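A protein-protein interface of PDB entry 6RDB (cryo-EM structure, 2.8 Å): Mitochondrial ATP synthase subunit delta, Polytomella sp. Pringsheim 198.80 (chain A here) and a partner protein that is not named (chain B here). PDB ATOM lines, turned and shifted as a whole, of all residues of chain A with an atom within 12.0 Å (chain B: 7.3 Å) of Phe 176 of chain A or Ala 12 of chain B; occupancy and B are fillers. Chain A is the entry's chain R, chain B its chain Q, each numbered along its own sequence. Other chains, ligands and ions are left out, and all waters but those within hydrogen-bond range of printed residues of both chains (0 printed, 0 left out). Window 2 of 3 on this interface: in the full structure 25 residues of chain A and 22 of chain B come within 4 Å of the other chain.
The backbone carbonyl oxygen (O) of Tyr 9 of chain B sits at hydrogen-bond distance from the backbone NH (N) of Met 14 of chain B, at 2.9 Å.
The side-chain hydroxyl of Ser 15 of chain B is in hydrogen-bond range of the backbone NH of Arg 18 of chain B (3.4 Å).
Glu 175 of chain A touches Ala 12 of chain B.
Ala 12 of chain B touches Phe 176 of chain A (O to CD1, 3.5 Å).
Met 14 of chain B touches Phe 176 of chain A.
Phe 176 of chain A touches Arg 18 of chain B (CZ to CD, 3.6 Å).
Phe 176 of chain A touches Lys 71 of chain B (CE2 to O, 3.5 Å).
O of Thr 72 of chain B touches CE2 of Phe 176 of chain A, 3.2 Å away.
Phe 176 of chain A touches Ala 73 of chain B (CD2 to N, 3.6 Å).
Phe 8 of chain B touches Ala 179 of chain A (CE1 to O, 3.4 Å).
Ala 12 of chain B touches Ala 179 of chain A (CB to CB, 3.95 Å).
Arg 182 of chain A touches Phe 8 of chain B.
Of chain B, only Ala 12, Met 14, Arg 18, Lys 71, Thr 72 and Ala 73 come within 4 Å of Phe 176 of chain A.
Ala 12 of chain B touches just these residues of chain A: Glu 175 (3.3 Å), Phe 176 (3.5 Å) and Ala 179 (3.95 Å).
No residue of chain A comes within 4 Å of Val 11 of chain B.
No residue of chain A comes within 4 Å of Gly 13 of chain B.
Of chain A, only Phe 176 (3.6 Å) comes within 4 Å of Met 14 of chain B.
No residue of chain A comes within 4 Å of Ser 15 of chain B.
Of chain A, only Phe 176 comes within 4 Å of Arg 18 of chain B.
Of the printed residues of chain A, Thr 72 of chain B touches Phe 176.
Of the printed residues of chain A, Lys 71 of chain B touches Phe 176.
Printed residues of chain B within 4 Å of Arg 182 of chain A: Phe 8.
Of the printed residues of chain A, Phe 8 of chain B touches Ala 179 and Arg 182.
Of the printed residues of chain B, Ala 183 of chain A touches Tyr 19 (3.7 Å).
Of the printed residues of chain B, Ala 179 of chain A touches Phe 8 (3.4 Å) and Ala 12 (3.95 Å).
Ala 180 of chain A touches none of the printed residues of chain B.
Pro 7 of chain B touches none of the printed residues of chain A.
The nearest residue of chain A that does not touch Ala 12 of chain B is Gln 178 of chain A (6.4 Å).
Of the 19 printed residues of chain B, 8 touch a printed residue of chain A.
Hydrophobic or aromatic side chains of chain A within 4 Å of the printed part of chain B: Phe 176, Ala 179 and Ala 183.
Along chain A the printed residues that touch a printed residue of chain B span positions 175 to 183.
Among the printed residues, no Asp or Glu carboxylate lies within 4 Å of a Lys or Arg side-chain nitrogen of the other chain.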
ATOM      1  N   ALA A 167      31.345   4.292 -12.923  1.00  0.00           N
ATOM      2  CA  ALA A 167      30.095   4.964 -13.251  1.00  0.00           C
ATOM      3  C   ALA A 167      29.996   5.338 -14.722  1.00  0.00           C
ATOM      4  O   ALA A 167      28.885   5.555 -15.216  1.00  0.00           O
ATOM      5  CB  ALA A 167      29.918   6.222 -12.398  1.00  0.00           C
ATOM      6  N   ALA A 170      28.565   1.351 -16.461  1.00  0.00           N
ATOM      7  CA  ALA A 170      27.257   0.717 -16.313  1.00  0.00           C
ATOM      8  C   ALA A 170      26.192   1.637 -16.894  1.00  0.00           C
ATOM      9  O   ALA A 170      25.683   2.529 -16.214  1.00  0.00           O
ATOM     10  CB  ALA A 170      26.979   0.396 -14.850  1.00  0.00           C
ATOM     11  N   GLN A 171      25.849   1.414 -18.163  1.00  0.00           N
ATOM     12  CA  GLN A 171      24.824   2.180 -18.872  1.00  0.00           C
ATOM     13  C   GLN A 171      23.662   1.257 -19.207  1.00  0.00           C
ATOM     14  O   GLN A 171      23.649   0.622 -20.274  1.00  0.00           O
ATOM     15  CB  GLN A 171      25.398   2.823 -20.134  1.00  0.00           C
ATOM     16  CG  GLN A 171      26.785   3.425 -19.950  1.00  0.00           C
ATOM     17  CD  GLN A 171      26.838   4.451 -18.831  1.00  0.00           C
ATOM     18  OE1 GLN A 171      25.916   5.247 -18.654  1.00  0.00           O
ATOM     19  NE2 GLN A 171      27.909   4.417 -18.053  1.00  0.00           N
ATOM     20  N   PRO A 172      22.664   1.142 -18.325  1.00  0.00           N
ATOM     21  CA  PRO A 172      21.513   0.285 -18.628  1.00  0.00           C
ATOM     22  C   PRO A 172      20.389   1.041 -19.317  1.00  0.00           C
ATOM     23  O   PRO A 172      20.426   2.271 -19.427  1.00  0.00           O
ATOM     24  CB  PRO A 172      21.079  -0.221 -17.244  1.00  0.00           C
ATOM     25  CG  PRO A 172      21.873   0.601 -16.226  1.00  0.00           C
ATOM     26  CD  PRO A 172      22.576   1.693 -16.966  1.00  0.00           C
ATOM     27  N   THR A 173      19.379   0.306 -19.785  1.00  0.00           N
ATOM     28  CA  THR A 173      18.174   0.928 -20.317  1.00  0.00           C
ATOM     29  C   THR A 173      17.195   1.329 -19.224  1.00  0.00           C
ATOM     30  O   THR A 173      16.207   2.012 -19.519  1.00  0.00           O
ATOM     31  CB  THR A 173      17.477  -0.010 -21.305  1.00  0.00           C
ATOM     32  OG1 THR A 173      16.405   0.687 -21.952  1.00  0.00           O
ATOM     33  CG2 THR A 173      16.918  -1.227 -20.582  1.00  0.00           C
ATOM     34  N   ASP A 174      17.447   0.921 -17.981  1.00  0.00           N
ATOM     35  CA  ASP A 174      16.600   1.303 -16.859  1.00  0.00           C
ATOM     36  C   ASP A 174      16.801   2.780 -16.552  1.00  0.00           C
ATOM     37  O   ASP A 174      17.890   3.190 -16.141  1.00  0.00           O
ATOM     38  CB  ASP A 174      16.931   0.448 -15.640  1.00  0.00           C
ATOM     39  CG  ASP A 174      16.000   0.706 -14.479  1.00  0.00           C
ATOM     40  OD1 ASP A 174      14.851   1.126 -14.722  1.00  0.00           O
ATOM     41  OD2 ASP A 174      16.423   0.497 -13.323  1.00  0.00           O
ATOM     42  N   GLU A 175      15.749   3.574 -16.748  1.00  0.00           N
ATOM     43  CA  GLU A 175      15.862   5.021 -16.628  1.00  0.00           C
ATOM     44  C   GLU A 175      15.990   5.485 -15.186  1.00  0.00           C
ATOM     45  O   GLU A 175      16.453   6.606 -14.955  1.00  0.00           O
ATOM     46  CB  GLU A 175      14.661   5.698 -17.292  1.00  0.00           C
ATOM     47  CG  GLU A 175      13.318   5.335 -16.689  1.00  0.00           C
ATOM     48  CD  GLU A 175      12.174   6.073 -17.349  1.00  0.00           C
ATOM     49  OE1 GLU A 175      12.445   6.940 -18.205  1.00  0.00           O
ATOM     50  OE2 GLU A 175      11.004   5.782 -17.020  1.00  0.00           O
ATOM     51  N   PHE A 176      15.602   4.657 -14.215  1.00  0.00           N
ATOM     52  CA  PHE A 176      15.810   5.027 -12.821  1.00  0.00           C
ATOM     53  C   PHE A 176      17.288   4.950 -12.465  1.00  0.00           C
ATOM     54  O   PHE A 176      17.833   5.860 -11.832  1.00  0.00           O
ATOM     55  CB  PHE A 176      15.005   4.113 -11.903  1.00  0.00           C
ATOM     56  CG  PHE A 176      14.803   4.662 -10.522  1.00  0.00           C
ATOM     57  CD1 PHE A 176      13.692   5.439 -10.246  1.00  0.00           C
ATOM     58  CD2 PHE A 176      15.735   4.453  -9.516  1.00  0.00           C
ATOM     59  CE1 PHE A 176      13.481   5.948  -8.986  1.00  0.00           C
ATOM     60  CE2 PHE A 176      15.537   4.974  -8.254  1.00  0.00           C
ATOM     61  CZ  PHE A 176      14.409   5.724  -7.992  1.00  0.00           C
ATOM     62  N   GLU A 177      17.952   3.865 -12.863  1.00  0.00           N
ATOM     63  CA  GLU A 177      19.382   3.744 -12.625  1.00  0.00           C
ATOM     64  C   GLU A 177      20.180   4.617 -13.582  1.00  0.00           C
ATOM     65  O   GLU A 177      21.306   5.010 -13.260  1.00  0.00           O
ATOM     66  CB  GLU A 177      19.815   2.284 -12.743  1.00  0.00           C
ATOM     67  CG  GLU A 177      20.898   1.871 -11.761  1.00  0.00           C
ATOM     68  CD  GLU A 177      22.286   2.268 -12.220  1.00  0.00           C
ATOM     69  OE1 GLU A 177      23.142   2.547 -11.360  1.00  0.00           O
ATOM     70  OE2 GLU A 177      22.515   2.315 -13.444  1.00  0.00           O
ATOM     71  N   GLN A 178      19.613   4.929 -14.752  1.00  0.00           N
ATOM     72  CA  GLN A 178      20.248   5.873 -15.663  1.00  0.00           C
ATOM     73  C   GLN A 178      20.318   7.265 -15.048  1.00  0.00           C
ATOM     74  O   GLN A 178      21.297   7.991 -15.250  1.00  0.00           O
ATOM     75  CB  GLN A 178      19.491   5.911 -16.991  1.00  0.00           C
ATOM     76  CG  GLN A 178      20.196   6.671 -18.102  1.00  0.00           C
ATOM     77  CD  GLN A 178      21.509   6.034 -18.490  1.00  0.00           C
ATOM     78  OE1 GLN A 178      22.570   6.639 -18.353  1.00  0.00           O
ATOM     79  NE2 GLN A 178      21.446   4.800 -18.976  1.00  0.00           N
ATOM     80  N   ALA A 179      19.290   7.645 -14.285  1.00  0.00           N
ATOM     81  CA  ALA A 179      19.317   8.922 -13.580  1.00  0.00           C
ATOM     82  C   ALA A 179      20.322   8.901 -12.438  1.00  0.00           C
ATOM     83  O   ALA A 179      21.014   9.896 -12.193  1.00  0.00           O
ATOM     84  CB  ALA A 179      17.920   9.264 -13.064  1.00  0.00           C
ATOM     85  N   ALA A 180      20.417   7.775 -11.727  1.00  0.00           N
ATOM     86  CA  ALA A 180      21.371   7.672 -10.628  1.00  0.00           C
ATOM     87  C   ALA A 180      22.799   7.527 -11.134  1.00  0.00           C
ATOM     88  O   ALA A 180      23.742   7.916 -10.439  1.00  0.00           O
ATOM     89  CB  ALA A 180      21.010   6.495  -9.724  1.00  0.00           C
ATOM     90  N   ASN A 181      22.980   6.975 -12.333  1.00  0.00           N
ATOM     91  CA  ASN A 181      24.310   6.948 -12.927  1.00  0.00           C
ATOM     92  C   ASN A 181      24.690   8.306 -13.494  1.00  0.00           C
ATOM     93  O   ASN A 181      25.871   8.667 -13.479  1.00  0.00           O
ATOM     94  CB  ASN A 181      24.385   5.876 -14.014  1.00  0.00           C
ATOM     95  CG  ASN A 181      25.774   5.732 -14.593  1.00  0.00           C
ATOM     96  OD1 ASN A 181      25.945   5.658 -15.805  1.00  0.00           O
ATOM     97  ND2 ASN A 181      26.775   5.700 -13.727  1.00  0.00           N
ATOM     98  N   ARG A 182      23.708   9.067 -13.989  1.00  0.00           N
ATOM     99  CA  ARG A 182      23.963  10.446 -14.393  1.00  0.00           C
ATOM    100  C   ARG A 182      24.383  11.294 -13.202  1.00  0.00           C
ATOM    101  O   ARG A 182      25.331  12.082 -13.292  1.00  0.00           O
ATOM    102  CB  ARG A 182      22.722  11.040 -15.062  1.00  0.00           C
ATOM    103  CG  ARG A 182      22.830  12.530 -15.345  1.00  0.00           C
ATOM    104  CD  ARG A 182      21.844  12.978 -16.405  1.00  0.00           C
ATOM    105  NE  ARG A 182      21.728  14.431 -16.446  1.00  0.00           N
ATOM    106  CZ  ARG A 182      20.892  15.089 -17.241  1.00  0.00           C
ATOM    107  NH1 ARG A 182      20.099  14.424 -18.064  1.00  0.00           N
ATOM    108  NH2 ARG A 182      20.850  16.412 -17.214  1.00  0.00           N
ATOM    109  N   ALA A 183      23.703  11.121 -12.064  1.00  0.00           N
ATOM    110  CA  ALA A 183      24.115  11.787 -10.836  1.00  0.00           C
ATOM    111  C   ALA A 183      25.439  11.243 -10.319  1.00  0.00           C
ATOM    112  O   ALA A 183      26.172  11.958  -9.630  1.00  0.00           O
ATOM    113  CB  ALA A 183      23.031  11.641  -9.775  1.00  0.00           C
ATOM    114  N   ALA A 184      25.763   9.990 -10.643  1.00  0.00           N
ATOM    115  CA  ALA A 184      27.070   9.450 -10.287  1.00  0.00           C
ATOM    116  C   ALA A 184      28.179  10.089 -11.113  1.00  0.00           C
ATOM    117  O   ALA A 184      29.295  10.281 -10.618  1.00  0.00           O
ATOM    118  CB  ALA A 184      27.083   7.935 -10.474  1.00  0.00           C
ATOM    119  N   ILE A 185      27.892  10.423 -12.371  1.00  0.00           N
ATOM    120  CA  ILE A 185      28.928  10.954 -13.251  1.00  0.00           C
ATOM    121  C   ILE A 185      29.250  12.400 -12.894  1.00  0.00           C
ATOM    122  O   ILE A 185      30.411  12.742 -12.646  1.00  0.00           O
ATOM    123  CB  ILE A 185      28.511  10.809 -14.728  1.00  0.00           C
ATOM    124  CG1 ILE A 185      28.590   9.344 -15.160  1.00  0.00           C
ATOM    125  CG2 ILE A 185      29.388  11.663 -15.627  1.00  0.00           C
ATOM    126  CD1 ILE A 185      27.663   8.988 -16.302  1.00  0.00           C
ATOM    127  N   ALA B   3       6.852  10.745 -18.931  1.00  0.00           N
ATOM    128  CA  ALA B   3       5.572  11.279 -18.469  1.00  0.00           C
ATOM    129  C   ALA B   3       5.637  12.463 -17.463  1.00  0.00           C
ATOM    130  O   ALA B   3       4.788  13.352 -17.556  1.00  0.00           O
ATOM    131  CB  ALA B   3       4.711  10.139 -17.895  1.00  0.00           C
ATOM    132  N   PRO B   4       6.585  12.519 -16.515  1.00  0.00           N
ATOM    133  CA  PRO B   4       6.755  13.773 -15.773  1.00  0.00           C
ATOM    134  C   PRO B   4       7.533  14.800 -16.578  1.00  0.00           C
ATOM    135  O   PRO B   4       8.263  14.473 -17.516  1.00  0.00           O
ATOM    136  CB  PRO B   4       7.534  13.353 -14.520  1.00  0.00           C
ATOM    137  CG  PRO B   4       7.362  11.897 -14.428  1.00  0.00           C
ATOM    138  CD  PRO B   4       7.348  11.449 -15.839  1.00  0.00           C
ATOM    139  N   PRO B   7      13.264  18.012 -14.086  1.00  0.00           N
ATOM    140  CA  PRO B   7      14.676  17.610 -14.165  1.00  0.00           C
ATOM    141  C   PRO B   7      14.875  16.138 -14.491  1.00  0.00           C
ATOM    142  O   PRO B   7      13.904  15.394 -14.646  1.00  0.00           O
ATOM    143  CB  PRO B   7      15.215  17.945 -12.770  1.00  0.00           C
ATOM    144  CG  PRO B   7      14.246  18.930 -12.208  1.00  0.00           C
ATOM    145  CD  PRO B   7      12.920  18.551 -12.761  1.00  0.00           C
ATOM    146  N   PHE B   8      16.134  15.703 -14.587  1.00  0.00           N
ATOM    147  CA  PHE B   8      16.409  14.350 -15.052  1.00  0.00           C
ATOM    148  C   PHE B   8      16.038  13.293 -14.026  1.00  0.00           C
ATOM    149  O   PHE B   8      15.702  12.169 -14.410  1.00  0.00           O
ATOM    150  CB  PHE B   8      17.879  14.209 -15.454  1.00  0.00           C
ATOM    151  CG  PHE B   8      18.853  14.285 -14.310  1.00  0.00           C
ATOM    152  CD1 PHE B   8      19.370  13.130 -13.743  1.00  0.00           C
ATOM    153  CD2 PHE B   8      19.297  15.510 -13.841  1.00  0.00           C
ATOM    154  CE1 PHE B   8      20.274  13.199 -12.708  1.00  0.00           C
ATOM    155  CE2 PHE B   8      20.205  15.585 -12.811  1.00  0.00           C
ATOM    156  CZ  PHE B   8      20.694  14.428 -12.244  1.00  0.00           C
ATOM    157  N   TYR B   9      16.084  13.621 -12.739  1.00  0.00           N
ATOM    158  CA  TYR B   9      15.602  12.682 -11.736  1.00  0.00           C
ATOM    159  C   TYR B   9      14.083  12.623 -11.712  1.00  0.00           C
ATOM    160  O   TYR B   9      13.514  11.548 -11.509  1.00  0.00           O
ATOM    161  CB  TYR B   9      16.144  13.048 -10.350  1.00  0.00           C
ATOM    162  CG  TYR B   9      16.048  14.512  -9.984  1.00  0.00           C
ATOM    163  CD1 TYR B   9      17.107  15.378 -10.220  1.00  0.00           C
ATOM    164  CD2 TYR B   9      14.910  15.021  -9.375  1.00  0.00           C
ATOM    165  CE1 TYR B   9      17.023  16.710  -9.881  1.00  0.00           C
ATOM    166  CE2 TYR B   9      14.818  16.350  -9.035  1.00  0.00           C
ATOM    167  CZ  TYR B   9      15.875  17.187  -9.289  1.00  0.00           C
ATOM    168  OH  TYR B   9      15.784  18.513  -8.947  1.00  0.00           O
ATOM    169  N   ARG B  10      13.416  13.749 -11.954  1.00  0.00           N
ATOM    170  CA  ARG B  10      11.967  13.808 -11.816  1.00  0.00           C
ATOM    171  C   ARG B  10      11.248  13.129 -12.974  1.00  0.00           C
ATOM    172  O   ARG B  10      10.215  12.486 -12.756  1.00  0.00           O
ATOM    173  CB  ARG B  10      11.523  15.264 -11.695  1.00  0.00           C
ATOM    174  CG  ARG B  10      10.092  15.444 -11.262  1.00  0.00           C
ATOM    175  CD  ARG B  10       9.871  14.904  -9.867  1.00  0.00           C
ATOM    176  NE  ARG B  10      10.438  15.773  -8.842  1.00  0.00           N
ATOM    177  CZ  ARG B  10      10.142  15.686  -7.550  1.00  0.00           C
ATOM    178  NH1 ARG B  10       9.278  14.774  -7.129  1.00  0.00           N
ATOM    179  NH2 ARG B  10      10.700  16.514  -6.680  1.00  0.00           N
ATOM    180  N   VAL B  11      11.775  13.253 -14.197  1.00  0.00           N
ATOM    181  CA  VAL B  11      11.179  12.587 -15.353  1.00  0.00           C
ATOM    182  C   VAL B  11      11.345  11.074 -15.240  1.00  0.00           C
ATOM    183  O   VAL B  11      10.449  10.308 -15.619  1.00  0.00           O
ATOM    184  CB  VAL B  11      11.788  13.152 -16.655  1.00  0.00           C
ATOM    185  CG1 VAL B  11      11.256  12.439 -17.888  1.00  0.00           C
ATOM    186  CG2 VAL B  11      11.497  14.637 -16.765  1.00  0.00           C
ATOM    187  N   ALA B  12      12.441  10.619 -14.638  1.00  0.00           N
ATOM    188  CA  ALA B  12      12.685   9.197 -14.438  1.00  0.00           C
ATOM    189  C   ALA B  12      11.963   8.623 -13.216  1.00  0.00           C
ATOM    190  O   ALA B  12      12.352   7.555 -12.733  1.00  0.00           O
ATOM    191  CB  ALA B  12      14.187   8.938 -14.323  1.00  0.00           C
ATOM    192  N   GLY B  13      10.932   9.302 -12.704  1.00  0.00           N
ATOM    193  CA  GLY B  13      10.142   8.816 -11.592  1.00  0.00           C
ATOM    194  C   GLY B  13      10.731   9.059 -10.223  1.00  0.00           C
ATOM    195  O   GLY B  13      10.011   8.926  -9.226  1.00  0.00           O
ATOM    196  N   MET B  14      12.006   9.416 -10.140  1.00  0.00           N
ATOM    197  CA  MET B  14      12.689   9.569  -8.868  1.00  0.00           C
ATOM    198  C   MET B  14      12.333  10.907  -8.233  1.00  0.00           C
ATOM    199  O   MET B  14      12.227  11.927  -8.917  1.00  0.00           O
ATOM    200  CB  MET B  14      14.196   9.448  -9.089  1.00  0.00           C
ATOM    201  CG  MET B  14      15.052   9.437  -7.855  1.00  0.00           C
ATOM    202  SD  MET B  14      16.776   9.702  -8.300  1.00  0.00           S
ATOM    203  CE  MET B  14      17.242   8.093  -8.901  1.00  0.00           C
ATOM    204  N   SER B  15      12.121  10.896  -6.922  1.00  0.00           N
ATOM    205  CA  SER B  15      11.860  12.127  -6.200  1.00  0.00           C
ATOM    206  C   SER B  15      13.166  12.871  -5.946  1.00  0.00           C
ATOM    207  O   SER B  15      14.262  12.344  -6.153  1.00  0.00           O
ATOM    208  CB  SER B  15      11.149  11.842  -4.880  1.00  0.00           C
ATOM    209  OG  SER B  15      11.960  11.055  -4.028  1.00  0.00           O
ATOM    210  N   ARG B  18      15.160  11.189  -2.807  1.00  0.00           N
ATOM    211  CA  ARG B  18      16.013  10.050  -3.114  1.00  0.00           C
ATOM    212  C   ARG B  18      17.189  10.465  -3.980  1.00  0.00           C
ATOM    213  O   ARG B  18      18.274   9.893  -3.859  1.00  0.00           O
ATOM    214  CB  ARG B  18      15.214   8.948  -3.806  1.00  0.00           C
ATOM    215  CG  ARG B  18      15.935   7.612  -3.847  1.00  0.00           C
ATOM    216  CD  ARG B  18      15.114   6.568  -4.554  1.00  0.00           C
ATOM    217  NE  ARG B  18      13.838   6.352  -3.890  1.00  0.00           N
ATOM    218  CZ  ARG B  18      13.639   5.468  -2.923  1.00  0.00           C
ATOM    219  NH1 ARG B  18      14.636   4.705  -2.497  1.00  0.00           N
ATOM    220  NH2 ARG B  18      12.436   5.354  -2.379  1.00  0.00           N
ATOM    221  N   TYR B  19      16.991  11.465  -4.840  1.00  0.00           N
ATOM    222  CA  TYR B  19      18.067  11.939  -5.701  1.00  0.00           C
ATOM    223  C   TYR B  19      19.166  12.608  -4.891  1.00  0.00           C
ATOM    224  O   TYR B  19      20.352  12.309  -5.067  1.00  0.00           O
ATOM    225  CB  TYR B  19      17.517  12.909  -6.745  1.00  0.00           C
ATOM    226  CG  TYR B  19      18.580  13.801  -7.338  1.00  0.00           C
ATOM    227  CD1 TYR B  19      18.634  15.154  -7.026  1.00  0.00           C
ATOM    228  CD2 TYR B  19      19.534  13.287  -8.200  1.00  0.00           C
ATOM    229  CE1 TYR B  19      19.608  15.963  -7.556  1.00  0.00           C
ATOM    230  CE2 TYR B  19      20.510  14.087  -8.733  1.00  0.00           C
ATOM    231  CZ  TYR B  19      20.543  15.424  -8.410  1.00  0.00           C
ATOM    232  OH  TYR B  19      21.520  16.227  -8.950  1.00  0.00           O
ATOM    233  N   ILE B  22      21.071  10.169  -2.832  1.00  0.00           N
ATOM    234  CA  ILE B  22      22.004   9.426  -3.679  1.00  0.00           C
ATOM    235  C   ILE B  22      23.289  10.218  -3.873  1.00  0.00           C
ATOM    236  O   ILE B  22      24.391   9.682  -3.715  1.00  0.00           O
ATOM    237  CB  ILE B  22      21.333   9.066  -5.020  1.00  0.00           C
ATOM    238  CG1 ILE B  22      20.518   7.785  -4.875  1.00  0.00           C
ATOM    239  CG2 ILE B  22      22.345   8.894  -6.136  1.00  0.00           C
ATOM    240  CD1 ILE B  22      19.586   7.529  -6.020  1.00  0.00           C
ATOM    241  N   PRO B  70      18.540   3.146  -1.437  1.00  0.00           N
ATOM    242  CA  PRO B  70      18.709   2.245  -2.587  1.00  0.00           C
ATOM    243  C   PRO B  70      18.845   3.007  -3.899  1.00  0.00           C
ATOM    244  O   PRO B  70      18.056   3.906  -4.199  1.00  0.00           O
ATOM    245  CB  PRO B  70      17.438   1.392  -2.560  1.00  0.00           C
ATOM    246  CG  PRO B  70      16.994   1.434  -1.151  1.00  0.00           C
ATOM    247  CD  PRO B  70      17.342   2.797  -0.654  1.00  0.00           C
ATOM    248  N   LYS B  71      19.861   2.628  -4.683  1.00  0.00           N
ATOM    249  CA  LYS B  71      20.086   3.253  -5.982  1.00  0.00           C
ATOM    250  C   LYS B  71      19.062   2.800  -7.009  1.00  0.00           C
ATOM    251  O   LYS B  71      18.683   3.579  -7.890  1.00  0.00           O
ATOM    252  CB  LYS B  71      21.492   2.931  -6.477  1.00  0.00           C
ATOM    253  CG  LYS B  71      22.599   3.472  -5.601  1.00  0.00           C
ATOM    254  CD  LYS B  71      23.892   2.712  -5.828  1.00  0.00           C
ATOM    255  CE  LYS B  71      25.049   3.353  -5.088  1.00  0.00           C
ATOM    256  NZ  LYS B  71      24.723   3.650  -3.667  1.00  0.00           N
ATOM    257  N   THR B  72      18.595   1.559  -6.909  1.00  0.00           N
ATOM    258  CA  THR B  72      17.637   1.026  -7.861  1.00  0.00           C
ATOM    259  C   THR B  72      16.232   1.532  -7.537  1.00  0.00           C
ATOM    260  O   THR B  72      16.014   2.273  -6.577  1.00  0.00           O
ATOM    261  CB  THR B  72      17.694  -0.500  -7.863  1.00  0.00           C
ATOM    262  OG1 THR B  72      17.025  -1.009  -6.701  1.00  0.00           O
ATOM    263  CG2 THR B  72      19.140  -0.966  -7.849  1.00  0.00           C
ATOM    264  N   ALA B  73      15.260   1.103  -8.337  1.00  0.00           N
ATOM    265  CA  ALA B  73      13.905   1.625  -8.233  1.00  0.00           C
ATOM    266  C   ALA B  73      13.185   1.021  -7.035  1.00  0.00           C
ATOM    267  O   ALA B  73      13.285  -0.182  -6.779  1.00  0.00           O
ATOM    268  CB  ALA B  73      13.126   1.348  -9.515  1.00  0.00           C
ATOM    269  N   ASN B  74      12.469   1.866  -6.299  1.00  0.00           N
ATOM    270  CA  ASN B  74      11.721   1.437  -5.124  1.00  0.00           C
ATOM    271  C   ASN B  74      10.365   0.867  -5.521  1.00  0.00           C
ATOM    272  O   ASN B  74       9.938  -0.166  -5.006  1.00  0.00           O
ATOM    273  CB  ASN B  74      11.533   2.604  -4.156  1.00  0.00           C
ATOM    274  CG  ASN B  74      11.098   2.155  -2.773  1.00  0.00           C
ATOM    275  OD1 ASN B  74      11.780   1.364  -2.122  1.00  0.00           O
ATOM    276  ND2 ASN B  74       9.960   2.662  -2.318  1.00  0.00           N
